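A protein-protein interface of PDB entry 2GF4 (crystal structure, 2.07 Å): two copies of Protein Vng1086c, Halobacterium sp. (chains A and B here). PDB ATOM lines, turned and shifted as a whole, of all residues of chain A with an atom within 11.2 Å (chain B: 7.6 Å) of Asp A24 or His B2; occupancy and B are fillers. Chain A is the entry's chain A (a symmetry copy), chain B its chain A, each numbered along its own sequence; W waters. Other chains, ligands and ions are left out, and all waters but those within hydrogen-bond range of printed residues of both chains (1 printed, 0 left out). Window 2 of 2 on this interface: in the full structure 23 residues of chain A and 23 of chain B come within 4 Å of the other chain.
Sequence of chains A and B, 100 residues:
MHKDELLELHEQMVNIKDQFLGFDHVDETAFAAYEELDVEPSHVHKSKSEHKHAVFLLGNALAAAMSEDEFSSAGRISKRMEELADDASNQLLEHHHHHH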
ATOM      1  N   ILE A  16     -11.790 -12.458 -17.423  1.00  0.00           N
ATOM      2  CA  ILE A  16     -11.929 -11.378 -18.416  1.00  0.00           C
ATOM      3  C   ILE A  16     -11.153 -10.141 -17.906  1.00  0.00           C
ATOM      4  O   ILE A  16     -10.347  -9.563 -18.647  1.00  0.00           O
ATOM      5  CB  ILE A  16     -13.426 -11.032 -18.606  1.00  0.00           C
ATOM      6  CG1 ILE A  16     -14.170 -12.198 -19.265  1.00  0.00           C
ATOM      7  CG2 ILE A  16     -13.555  -9.830 -19.451  1.00  0.00           C
ATOM      8  CD1 ILE A  16     -13.889 -12.357 -20.647  1.00  0.00           C
ATOM      9  N   LYS A  17     -11.397  -9.733 -16.657  1.00  0.00           N
ATOM     10  CA  LYS A  17     -10.712  -8.595 -16.062  1.00  0.00           C
ATOM     11  C   LYS A  17      -9.206  -8.702 -16.179  1.00  0.00           C
ATOM     12  O   LYS A  17      -8.563  -7.726 -16.553  1.00  0.00           O
ATOM     13  CB  LYS A  17     -11.044  -8.514 -14.596  1.00  0.00           C
ATOM     14  CG  LYS A  17     -10.195  -7.479 -13.959  1.00  0.00           C
ATOM     15  CD  LYS A  17     -10.875  -6.896 -12.813  1.00  0.00           C
ATOM     16  CE  LYS A  17     -10.620  -7.732 -11.645  1.00  0.00           C
ATOM     17  NZ  LYS A  17      -9.189  -7.829 -11.356  1.00  0.00           N
ATOM     18  N   ASP A  18      -8.643  -9.866 -15.844  1.00  0.00           N
ATOM     19  CA  ASP A  18      -7.198 -10.006 -15.925  1.00  0.00           C
ATOM     20  C   ASP A  18      -6.740  -9.908 -17.357  1.00  0.00           C
ATOM     21  O   ASP A  18      -5.716  -9.275 -17.616  1.00  0.00           O
ATOM     22  CB  ASP A  18      -6.785 -11.284 -15.227  1.00  0.00           C
ATOM     23  CG  ASP A  18      -6.945 -11.159 -13.713  1.00  0.00           C
ATOM     24  OD1 ASP A  18      -6.892 -10.030 -13.177  1.00  0.00           O
ATOM     25  OD2 ASP A  18      -7.115 -12.168 -13.024  1.00  0.00           O
ATOM     26  N   GLN A  19      -7.495 -10.511 -18.278  1.00  0.00           N
ATOM     27  CA  GLN A  19      -7.230 -10.452 -19.716  1.00  0.00           C
ATOM     28  C   GLN A  19      -7.160  -8.964 -20.123  1.00  0.00           C
ATOM     29  O   GLN A  19      -6.168  -8.543 -20.716  1.00  0.00           O
ATOM     30  CB  GLN A  19      -8.393 -11.111 -20.447  1.00  0.00           C
ATOM     31  CG  GLN A  19      -8.109 -11.279 -21.898  1.00  0.00           C
ATOM     32  CD  GLN A  19      -9.252 -11.876 -22.679  1.00  0.00           C
ATOM     33  OE1 GLN A  19     -10.341 -12.126 -22.157  1.00  0.00           O
ATOM     34  NE2 GLN A  19      -8.998 -12.093 -23.948  1.00  0.00           N
ATOM     35  N   PHE A  20      -8.211  -8.182 -19.813  1.00  0.00           N
ATOM     36  CA  PHE A  20      -8.275  -6.756 -20.148  1.00  0.00           C
ATOM     37  C   PHE A  20      -7.082  -5.972 -19.580  1.00  0.00           C
ATOM     38  O   PHE A  20      -6.470  -5.201 -20.321  1.00  0.00           O
ATOM     39  CB  PHE A  20      -9.587  -6.167 -19.603  1.00  0.00           C
ATOM     40  CG  PHE A  20      -9.725  -4.678 -19.774  1.00  0.00           C
ATOM     41  CD1 PHE A  20     -10.313  -4.126 -20.905  1.00  0.00           C
ATOM     42  CD2 PHE A  20      -9.293  -3.821 -18.774  1.00  0.00           C
ATOM     43  CE1 PHE A  20     -10.474  -2.750 -21.006  1.00  0.00           C
ATOM     44  CE2 PHE A  20      -9.459  -2.454 -18.887  1.00  0.00           C
ATOM     45  CZ  PHE A  20     -10.044  -1.922 -19.997  1.00  0.00           C
ATOM     46  N   LEU A  21      -6.745  -6.182 -18.302  1.00  0.00           N
ATOM     47  CA  LEU A  21      -5.647  -5.443 -17.695  1.00  0.00           C
ATOM     48  C   LEU A  21      -4.339  -5.786 -18.345  1.00  0.00           C
ATOM     49  O   LEU A  21      -3.370  -5.042 -18.217  1.00  0.00           O
ATOM     50  CB  LEU A  21      -5.618  -5.695 -16.195  1.00  0.00           C
ATOM     51  CG  LEU A  21      -6.831  -5.087 -15.468  1.00  0.00           C
ATOM     52  CD1 LEU A  21      -6.775  -5.649 -14.108  1.00  0.00           C
ATOM     53  CD2 LEU A  21      -6.827  -3.564 -15.411  1.00  0.00           C
ATOM     54  N   GLY A  22      -4.310  -6.908 -19.060  1.00  0.00           N
ATOM     55  CA  GLY A  22      -3.100  -7.264 -19.769  1.00  0.00           C
ATOM     56  C   GLY A  22      -3.018  -6.552 -21.122  1.00  0.00           C
ATOM     57  O   GLY A  22      -1.982  -6.652 -21.781  1.00  0.00           O
ATOM     58  N   PHE A  23      -4.030  -5.813 -21.554  1.00  0.00           N
ATOM     59  CA  PHE A  23      -3.909  -5.191 -22.869  1.00  0.00           C
ATOM     60  C   PHE A  23      -3.046  -3.942 -22.934  1.00  0.00           C
ATOM     61  O   PHE A  23      -2.593  -3.393 -21.928  1.00  0.00           O
ATOM     62  CB  PHE A  23      -5.291  -4.875 -23.439  1.00  0.00           C
ATOM     63  CG  PHE A  23      -6.119  -6.088 -23.746  1.00  0.00           C
ATOM     64  CD1 PHE A  23      -5.530  -7.315 -24.022  1.00  0.00           C
ATOM     65  CD2 PHE A  23      -7.489  -5.998 -23.790  1.00  0.00           C
ATOM     66  CE1 PHE A  23      -6.319  -8.416 -24.308  1.00  0.00           C
ATOM     67  CE2 PHE A  23      -8.258  -7.092 -24.073  1.00  0.00           C
ATOM     68  CZ  PHE A  23      -7.678  -8.294 -24.339  1.00  0.00           C
ATOM     69  N   ASP A  24      -2.800  -3.524 -24.158  1.00  0.00           N
ATOM     70  CA  ASP A  24      -2.017  -2.349 -24.415  1.00  0.00           C
ATOM     71  C   ASP A  24      -2.788  -1.093 -24.089  1.00  0.00           C
ATOM     72  O   ASP A  24      -3.943  -0.937 -24.495  1.00  0.00           O
ATOM     73  CB  ASP A  24      -1.692  -2.273 -25.875  1.00  0.00           C
ATOM     74  CG  ASP A  24      -0.437  -1.524 -26.125  1.00  0.00           C
ATOM     75  OD1 ASP A  24       0.557  -1.860 -25.464  1.00  0.00           O
ATOM     76  OD2 ASP A  24      -0.404  -0.610 -26.961  1.00  0.00           O
ATOM     77  N   HIS A  25      -2.142  -0.176 -23.393  1.00  0.00           N
ATOM     78  CA  HIS A  25      -2.789   1.077 -23.105  1.00  0.00           C
ATOM     79  C   HIS A  25      -4.216   1.019 -22.674  1.00  0.00           C
ATOM     80  O   HIS A  25      -5.082   1.641 -23.294  1.00  0.00           O
ATOM     81  CB  HIS A  25      -2.681   1.983 -24.315  1.00  0.00           C
ATOM     82  CG  HIS A  25      -1.313   2.558 -24.501  1.00  0.00           C
ATOM     83  ND1 HIS A  25      -0.198   1.771 -24.674  1.00  0.00           N
ATOM     84  CD2 HIS A  25      -0.881   3.838 -24.516  1.00  0.00           C
ATOM     85  CE1 HIS A  25       0.863   2.543 -24.796  1.00  0.00           C
ATOM     86  NE2 HIS A  25       0.476   3.801 -24.701  1.00  0.00           N
ATOM     87  N   VAL A  26      -4.473   0.288 -21.613  1.00  0.00           N
ATOM     88  CA  VAL A  26      -5.827   0.227 -21.108  1.00  0.00           C
ATOM     89  C   VAL A  26      -5.938   0.996 -19.802  1.00  0.00           C
ATOM     90  O   VAL A  26      -4.933   1.345 -19.176  1.00  0.00           O
ATOM     91  CB  VAL A  26      -6.254  -1.200 -20.844  1.00  0.00           C
ATOM     92  CG1 VAL A  26      -6.355  -1.920 -22.118  1.00  0.00           C
ATOM     93  CG2 VAL A  26      -5.248  -1.889 -20.030  1.00  0.00           C
ATOM     94  N   ASP A  27      -7.159   1.291 -19.397  1.00  0.00           N
ATOM     95  CA  ASP A  27      -7.355   1.990 -18.147  1.00  0.00           C
ATOM     96  C   ASP A  27      -7.254   0.987 -16.986  1.00  0.00           C
ATOM     97  O   ASP A  27      -8.174   0.183 -16.729  1.00  0.00           O
ATOM     98  CB  ASP A  27      -8.696   2.662 -18.134  1.00  0.00           C
ATOM     99  CG  ASP A  27      -8.996   3.266 -16.809  1.00  0.00           C
ATOM    100  OD1 ASP A  27      -8.026   3.539 -16.075  1.00  0.00           O
ATOM    101  OD2 ASP A  27     -10.165   3.482 -16.468  1.00  0.00           O
ATOM    102  N   GLU A  28      -6.163   1.079 -16.259  1.00  0.00           N
ATOM    103  CA  GLU A  28      -5.925   0.138 -15.201  1.00  0.00           C
ATOM    104  C   GLU A  28      -6.765   0.355 -13.970  1.00  0.00           C
ATOM    105  O   GLU A  28      -6.788  -0.496 -13.081  1.00  0.00           O
ATOM    106  CB  GLU A  28      -4.434   0.106 -14.910  1.00  0.00           C
ATOM    107  CG  GLU A  28      -3.910   1.351 -14.251  1.00  0.00           C
ATOM    108  CD  GLU A  28      -3.820   2.560 -15.174  1.00  0.00           C
ATOM    109  OE1 GLU A  28      -4.032   2.430 -16.398  1.00  0.00           O
ATOM    110  OE2 GLU A  28      -3.511   3.665 -14.680  1.00  0.00           O
ATOM    111  N   ALA A  65     -15.458   0.741 -19.752  1.00  0.00           N
ATOM    112  CA  ALA A  65     -14.148   0.902 -20.361  1.00  0.00           C
ATOM    113  C   ALA A  65     -14.245   0.926 -21.895  1.00  0.00           C
ATOM    114  O   ALA A  65     -13.453   1.603 -22.539  1.00  0.00           O
ATOM    115  CB  ALA A  65     -13.282  -0.198 -19.928  1.00  0.00           C
ATOM    116  N   MET A  66     -15.175   0.177 -22.486  1.00  0.00           N
ATOM    117  CA  MET A  66     -15.329   0.218 -23.944  1.00  0.00           C
ATOM    118  C   MET A  66     -15.850   1.580 -24.332  1.00  0.00           C
ATOM    119  O   MET A  66     -15.474   2.113 -25.370  1.00  0.00           O
ATOM    120  CB  MET A  66     -16.377  -0.755 -24.384  1.00  0.00           C
ATOM    121  CG  MET A  66     -15.990  -2.168 -24.062  1.00  0.00           C
ATOM    122  SD  MET A  66     -14.213  -2.793 -24.934  1.00  0.00           S
ATOM    123  CE  MET A  66     -12.848  -2.870 -23.404  1.00  0.00           C
ATOM    124  N   ASP A  69     -13.067   4.184 -24.092  1.00  0.00           N
ATOM    125  CA  ASP A  69     -12.132   4.024 -25.163  1.00  0.00           C
ATOM    126  C   ASP A  69     -12.713   4.572 -26.475  1.00  0.00           C
ATOM    127  O   ASP A  69     -11.977   5.178 -27.250  1.00  0.00           O
ATOM    128  CB  ASP A  69     -11.804   2.570 -25.290  1.00  0.00           C
ATOM    129  CG  ASP A  69     -10.867   2.312 -26.397  1.00  0.00           C
ATOM    130  OD1 ASP A  69      -9.837   1.684 -26.169  1.00  0.00           O
ATOM    131  OD2 ASP A  69     -11.143   2.759 -27.525  1.00  0.00           O
ATOM    132  N   SER A  72     -12.978   8.331 -26.391  1.00  0.00           N
ATOM    133  CA  SER A  72     -11.684   8.990 -26.598  1.00  0.00           C
ATOM    134  C   SER A  72     -10.933   8.709 -27.903  1.00  0.00           C
ATOM    135  O   SER A  72      -9.828   9.227 -28.093  1.00  0.00           O
ATOM    136  CB  SER A  72     -10.780   8.748 -25.404  1.00  0.00           C
ATOM    137  OG  SER A  72      -9.601   8.055 -25.768  1.00  0.00           O
ATOM    138  N   SER A  73     -11.495   7.909 -28.804  1.00  0.00           N
ATOM    139  CA  SER A  73     -10.801   7.737 -30.072  1.00  0.00           C
ATOM    140  C   SER A  73     -11.719   8.283 -31.144  1.00  0.00           C
ATOM    141  O   SER A  73     -11.416   9.318 -31.739  1.00  0.00           O
ATOM    142  CB  SER A  73     -10.430   6.282 -30.333  1.00  0.00           C
ATOM    143  OG  SER A  73     -11.536   5.412 -30.184  1.00  0.00           O
ATOM    144  N   MET B   1      -5.519  -0.304 -26.868  1.00  0.00           N
ATOM    145  CA  MET B   1      -5.920  -1.728 -27.045  1.00  0.00           C
ATOM    146  C   MET B   1      -5.833  -2.125 -28.518  1.00  0.00           C
ATOM    147  O   MET B   1      -6.494  -1.538 -29.369  1.00  0.00           O
ATOM    148  CB  MET B   1      -7.344  -1.932 -26.515  1.00  0.00           C
ATOM    149  CG  MET B   1      -7.917  -3.321 -26.738  1.00  0.00           C
ATOM    150  SD  MET B   1      -9.492  -3.641 -25.654  1.00  0.00           S
ATOM    151  CE  MET B   1     -10.567  -2.155 -26.257  1.00  0.00           C
ATOM    152  N   HIS B   2      -5.006  -3.121 -28.813  1.00  0.00           N
ATOM    153  CA  HIS B   2      -4.829  -3.585 -30.190  1.00  0.00           C
ATOM    154  C   HIS B   2      -6.064  -4.297 -30.731  1.00  0.00           C
ATOM    155  O   HIS B   2      -6.943  -4.686 -29.962  1.00  0.00           O
ATOM    156  CB  HIS B   2      -3.622  -4.514 -30.264  1.00  0.00           C
ATOM    157  CG  HIS B   2      -2.328  -3.830 -29.962  1.00  0.00           C
ATOM    158  ND1 HIS B   2      -1.912  -2.704 -30.639  1.00  0.00           N
ATOM    159  CD2 HIS B   2      -1.377  -4.085 -29.032  1.00  0.00           C
ATOM    160  CE1 HIS B   2      -0.761  -2.291 -30.135  1.00  0.00           C
ATOM    161  NE2 HIS B   2      -0.415  -3.112 -29.160  1.00  0.00           N
ATOM    162  N   LYS B   3      -6.138  -4.467 -32.049  1.00  0.00           N
ATOM    163  CA  LYS B   3      -7.294  -5.145 -32.619  1.00  0.00           C
ATOM    164  C   LYS B   3      -7.307  -6.621 -32.231  1.00  0.00           C
ATOM    165  O   LYS B   3      -8.356  -7.149 -31.862  1.00  0.00           O
ATOM    166  CB  LYS B   3      -7.354  -4.994 -34.142  1.00  0.00           C
ATOM    167  CG  LYS B   3      -8.650  -5.578 -34.708  1.00  0.00           C
ATOM    168  CD  LYS B   3      -8.944  -5.180 -36.147  1.00  0.00           C
ATOM    169  CE  LYS B   3     -10.286  -5.765 -36.581  1.00  0.00           C
ATOM    170  NZ  LYS B   3     -10.676  -5.386 -37.966  1.00  0.00           N
ATOM    171  N   ASP B   4      -6.162  -7.298 -32.311  1.00  0.00           N
ATOM    172  CA  ASP B   4      -6.133  -8.717 -31.894  1.00  0.00           C
ATOM    173  C   ASP B   4      -6.533  -8.874 -30.404  1.00  0.00           C
ATOM    174  O   ASP B   4      -7.079  -9.915 -30.034  1.00  0.00           O
ATOM    175  CB  ASP B   4      -4.737  -9.285 -32.089  1.00  0.00           C
ATOM    176  CG  ASP B   4      -4.421  -9.557 -33.553  1.00  0.00           C
ATOM    177  OD1 ASP B   4      -5.281  -9.287 -34.420  1.00  0.00           O
ATOM    178  OD2 ASP B   4      -3.319 -10.039 -33.847  1.00  0.00           O
ATOM    179  N   GLU B   5      -6.219  -7.906 -29.542  1.00  0.00           N
ATOM    180  CA  GLU B   5      -6.614  -8.027 -28.129  1.00  0.00           C
ATOM    181  C   GLU B   5      -8.134  -7.852 -28.055  1.00  0.00           C
ATOM    182  O   GLU B   5      -8.795  -8.573 -27.319  1.00  0.00           O
ATOM    183  CB  GLU B   5      -5.937  -6.951 -27.278  1.00  0.00           C
ATOM    184  CG  GLU B   5      -4.417  -7.108 -27.220  1.00  0.00           C
ATOM    185  CD  GLU B   5      -3.709  -5.919 -26.592  1.00  0.00           C
ATOM    186  OE1 GLU B   5      -4.088  -4.742 -26.812  1.00  0.00           O
ATOM    187  OE2 GLU B   5      -2.713  -6.142 -25.880  1.00  0.00           O
ATOM    188  N   LEU B   6      -8.700  -6.911 -28.798  1.00  0.00           N
ATOM    189  CA  LEU B   6     -10.143  -6.706 -28.749  1.00  0.00           C
ATOM    190  C   LEU B   6     -10.910  -7.912 -29.296  1.00  0.00           C
ATOM    191  O   LEU B   6     -11.976  -8.242 -28.766  1.00  0.00           O
ATOM    192  CB  LEU B   6     -10.457  -5.448 -29.533  1.00  0.00           C
ATOM    193  CG  LEU B   6     -11.891  -4.920 -29.620  1.00  0.00           C
ATOM    194  CD1 LEU B   6     -12.460  -4.568 -28.274  1.00  0.00           C
ATOM    195  CD2 LEU B   6     -11.844  -3.710 -30.479  1.00  0.00           C
ATOM    196  N   LEU B   7     -10.401  -8.551 -30.353  1.00  0.00           N
ATOM    197  CA  LEU B   7     -11.077  -9.732 -30.904  1.00  0.00           C
ATOM    198  C   LEU B   7     -11.075 -10.828 -29.839  1.00  0.00           C
ATOM    199  O   LEU B   7     -12.102 -11.483 -29.635  1.00  0.00           O
ATOM    200  CB  LEU B   7     -10.363 -10.228 -32.179  1.00  0.00           C
ATOM    201  CG  LEU B   7     -10.520  -9.237 -33.373  1.00  0.00           C
ATOM    202  CD1 LEU B   7      -9.674  -9.712 -34.514  1.00  0.00           C
ATOM    203  CD2 LEU B   7     -11.963  -9.097 -33.845  1.00  0.00           C
ATOM    204  N   GLU B   8      -9.938 -11.004 -29.151  1.00  0.00           N
ATOM    205  CA  GLU B   8      -9.816 -12.018 -28.108  1.00  0.00           C
ATOM    206  C   GLU B   8     -10.758 -11.696 -26.953  1.00  0.00           C
ATOM    207  O   GLU B   8     -11.322 -12.616 -26.357  1.00  0.00           O
ATOM    208  CB  GLU B   8      -8.357 -12.103 -27.647  1.00  0.00           C
ATOM    209  CG  GLU B   8      -7.481 -12.812 -28.698  1.00  0.00           C
ATOM    210  CD  GLU B   8      -5.991 -12.787 -28.383  1.00  0.00           C
ATOM    211  OE1 GLU B   8      -5.510 -13.662 -27.635  1.00  0.00           O
ATOM    212  OE2 GLU B   8      -5.286 -11.888 -28.890  1.00  0.00           O
ATOM    213  N   LYS B  48     -12.597  -1.941 -35.374  1.00  0.00           N
ATOM    214  CA  LYS B  48     -12.298  -1.944 -33.944  1.00  0.00           C
ATOM    215  C   LYS B  48     -13.535  -1.377 -33.241  1.00  0.00           C
ATOM    216  O   LYS B  48     -13.915  -1.856 -32.174  1.00  0.00           O
ATOM    217  CB  LYS B  48     -11.146  -1.008 -33.659  1.00  0.00           C
ATOM    218  CG  LYS B  48      -9.836  -1.706 -33.521  1.00  0.00           C
ATOM    219  CD  LYS B  48      -8.791  -0.657 -33.190  1.00  0.00           C
ATOM    220  CE  LYS B  48      -7.888  -1.122 -32.052  1.00  0.00           C
ATOM    221  NZ  LYS B  48      -7.483  -0.056 -31.075  1.00  0.00           N
HETATM  222  O   HOH W   1      -3.182   0.116 -28.117  1.00  0.00           O
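Of the 18 printed residues of chain A, 5 touch a printed residue of chain B.
Hydrophobic or aromatic side chains of chain A that line the printed part of chain B: Phe A23 and Met A66.
Along chain A the printed residues that touch a printed residue of chain B span positions 19 to 69.
Among the printed residues, no Asp or Glu carboxylate lies within 4 Å of a Lys or Arg side-chain nitrogen of the other chain.
O of Glu B8 is in hydrogen-bond range of NE2 of Gln A19 (3.4 Å).
The backbone NH (N) of Asp A24 is in hydrogen-bond range of the side-chain carboxylate (OE2) of Glu B5 (3.1 Å).
NE2 of His B2 lies within hydrogen-bond range of OD2 of Asp A24 (3.3 Å).
N of Met B1 lies within hydrogen-bond range of O of Asp A24, at 2.9 Å.
The side-chain hydroxyl (OG) of Ser A73 lies within hydrogen-bond range of the backbone carbonyl oxygen (O) of Asp A69, at 3.0 Å.
N of His B2 sits at hydrogen-bond distance from OE1 of Glu B5.
The side-chain amino group of Lys B48 lies within hydrogen-bond range of the backbone carbonyl oxygen of Met B1.
A ring nitrogen (ND1) of His A25 lies within hydrogen-bond range of the side-chain carboxylate (OD2) of Asp A24 (3.3 Å).
Water W1 bridges the backbone NH (N) of Met B1 and the side-chain carboxylate (OD2) of Asp A24.
Asp A24 touches just these residues of chain B: Met B1 (2.9 Å), His B2 (3.3 Å) and Glu B5 (3.1 Å).
Printed residues of chain B within 4 Å of Asp A69: Met B1.
His B2 touches one residue of chain A.
No residue of chain A comes within 4 Å of Asp B4.
Of chain A, only Phe A23 (3.2 Å) and Asp A24 (3.1 Å) come within 4 Å of Glu B5.
Of the printed residues of chain A, Glu B8 touches Gln A19 (3.4 Å).
The nearest residue of chain A that does not touch His B2 is Phe A23 (5.7 Å).
The nearest printed residue of chain A that does not touch Glu B8 is Phe A23 (5.1 Å).
No position is printed for both chains.
Of the 8 pairs that touch across the chains among the printed residues, none has its exchanged pair printed and touching as well.
Among the printed residues, merely in contact across the chains: Phe A23 with Glu B5 (3.2 Å), Phe A23 with Met B1 (3.6 Å), Met A66 with Met B1 (3.7 Å) and Asp A69 with Met B1 (3.9 Å).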
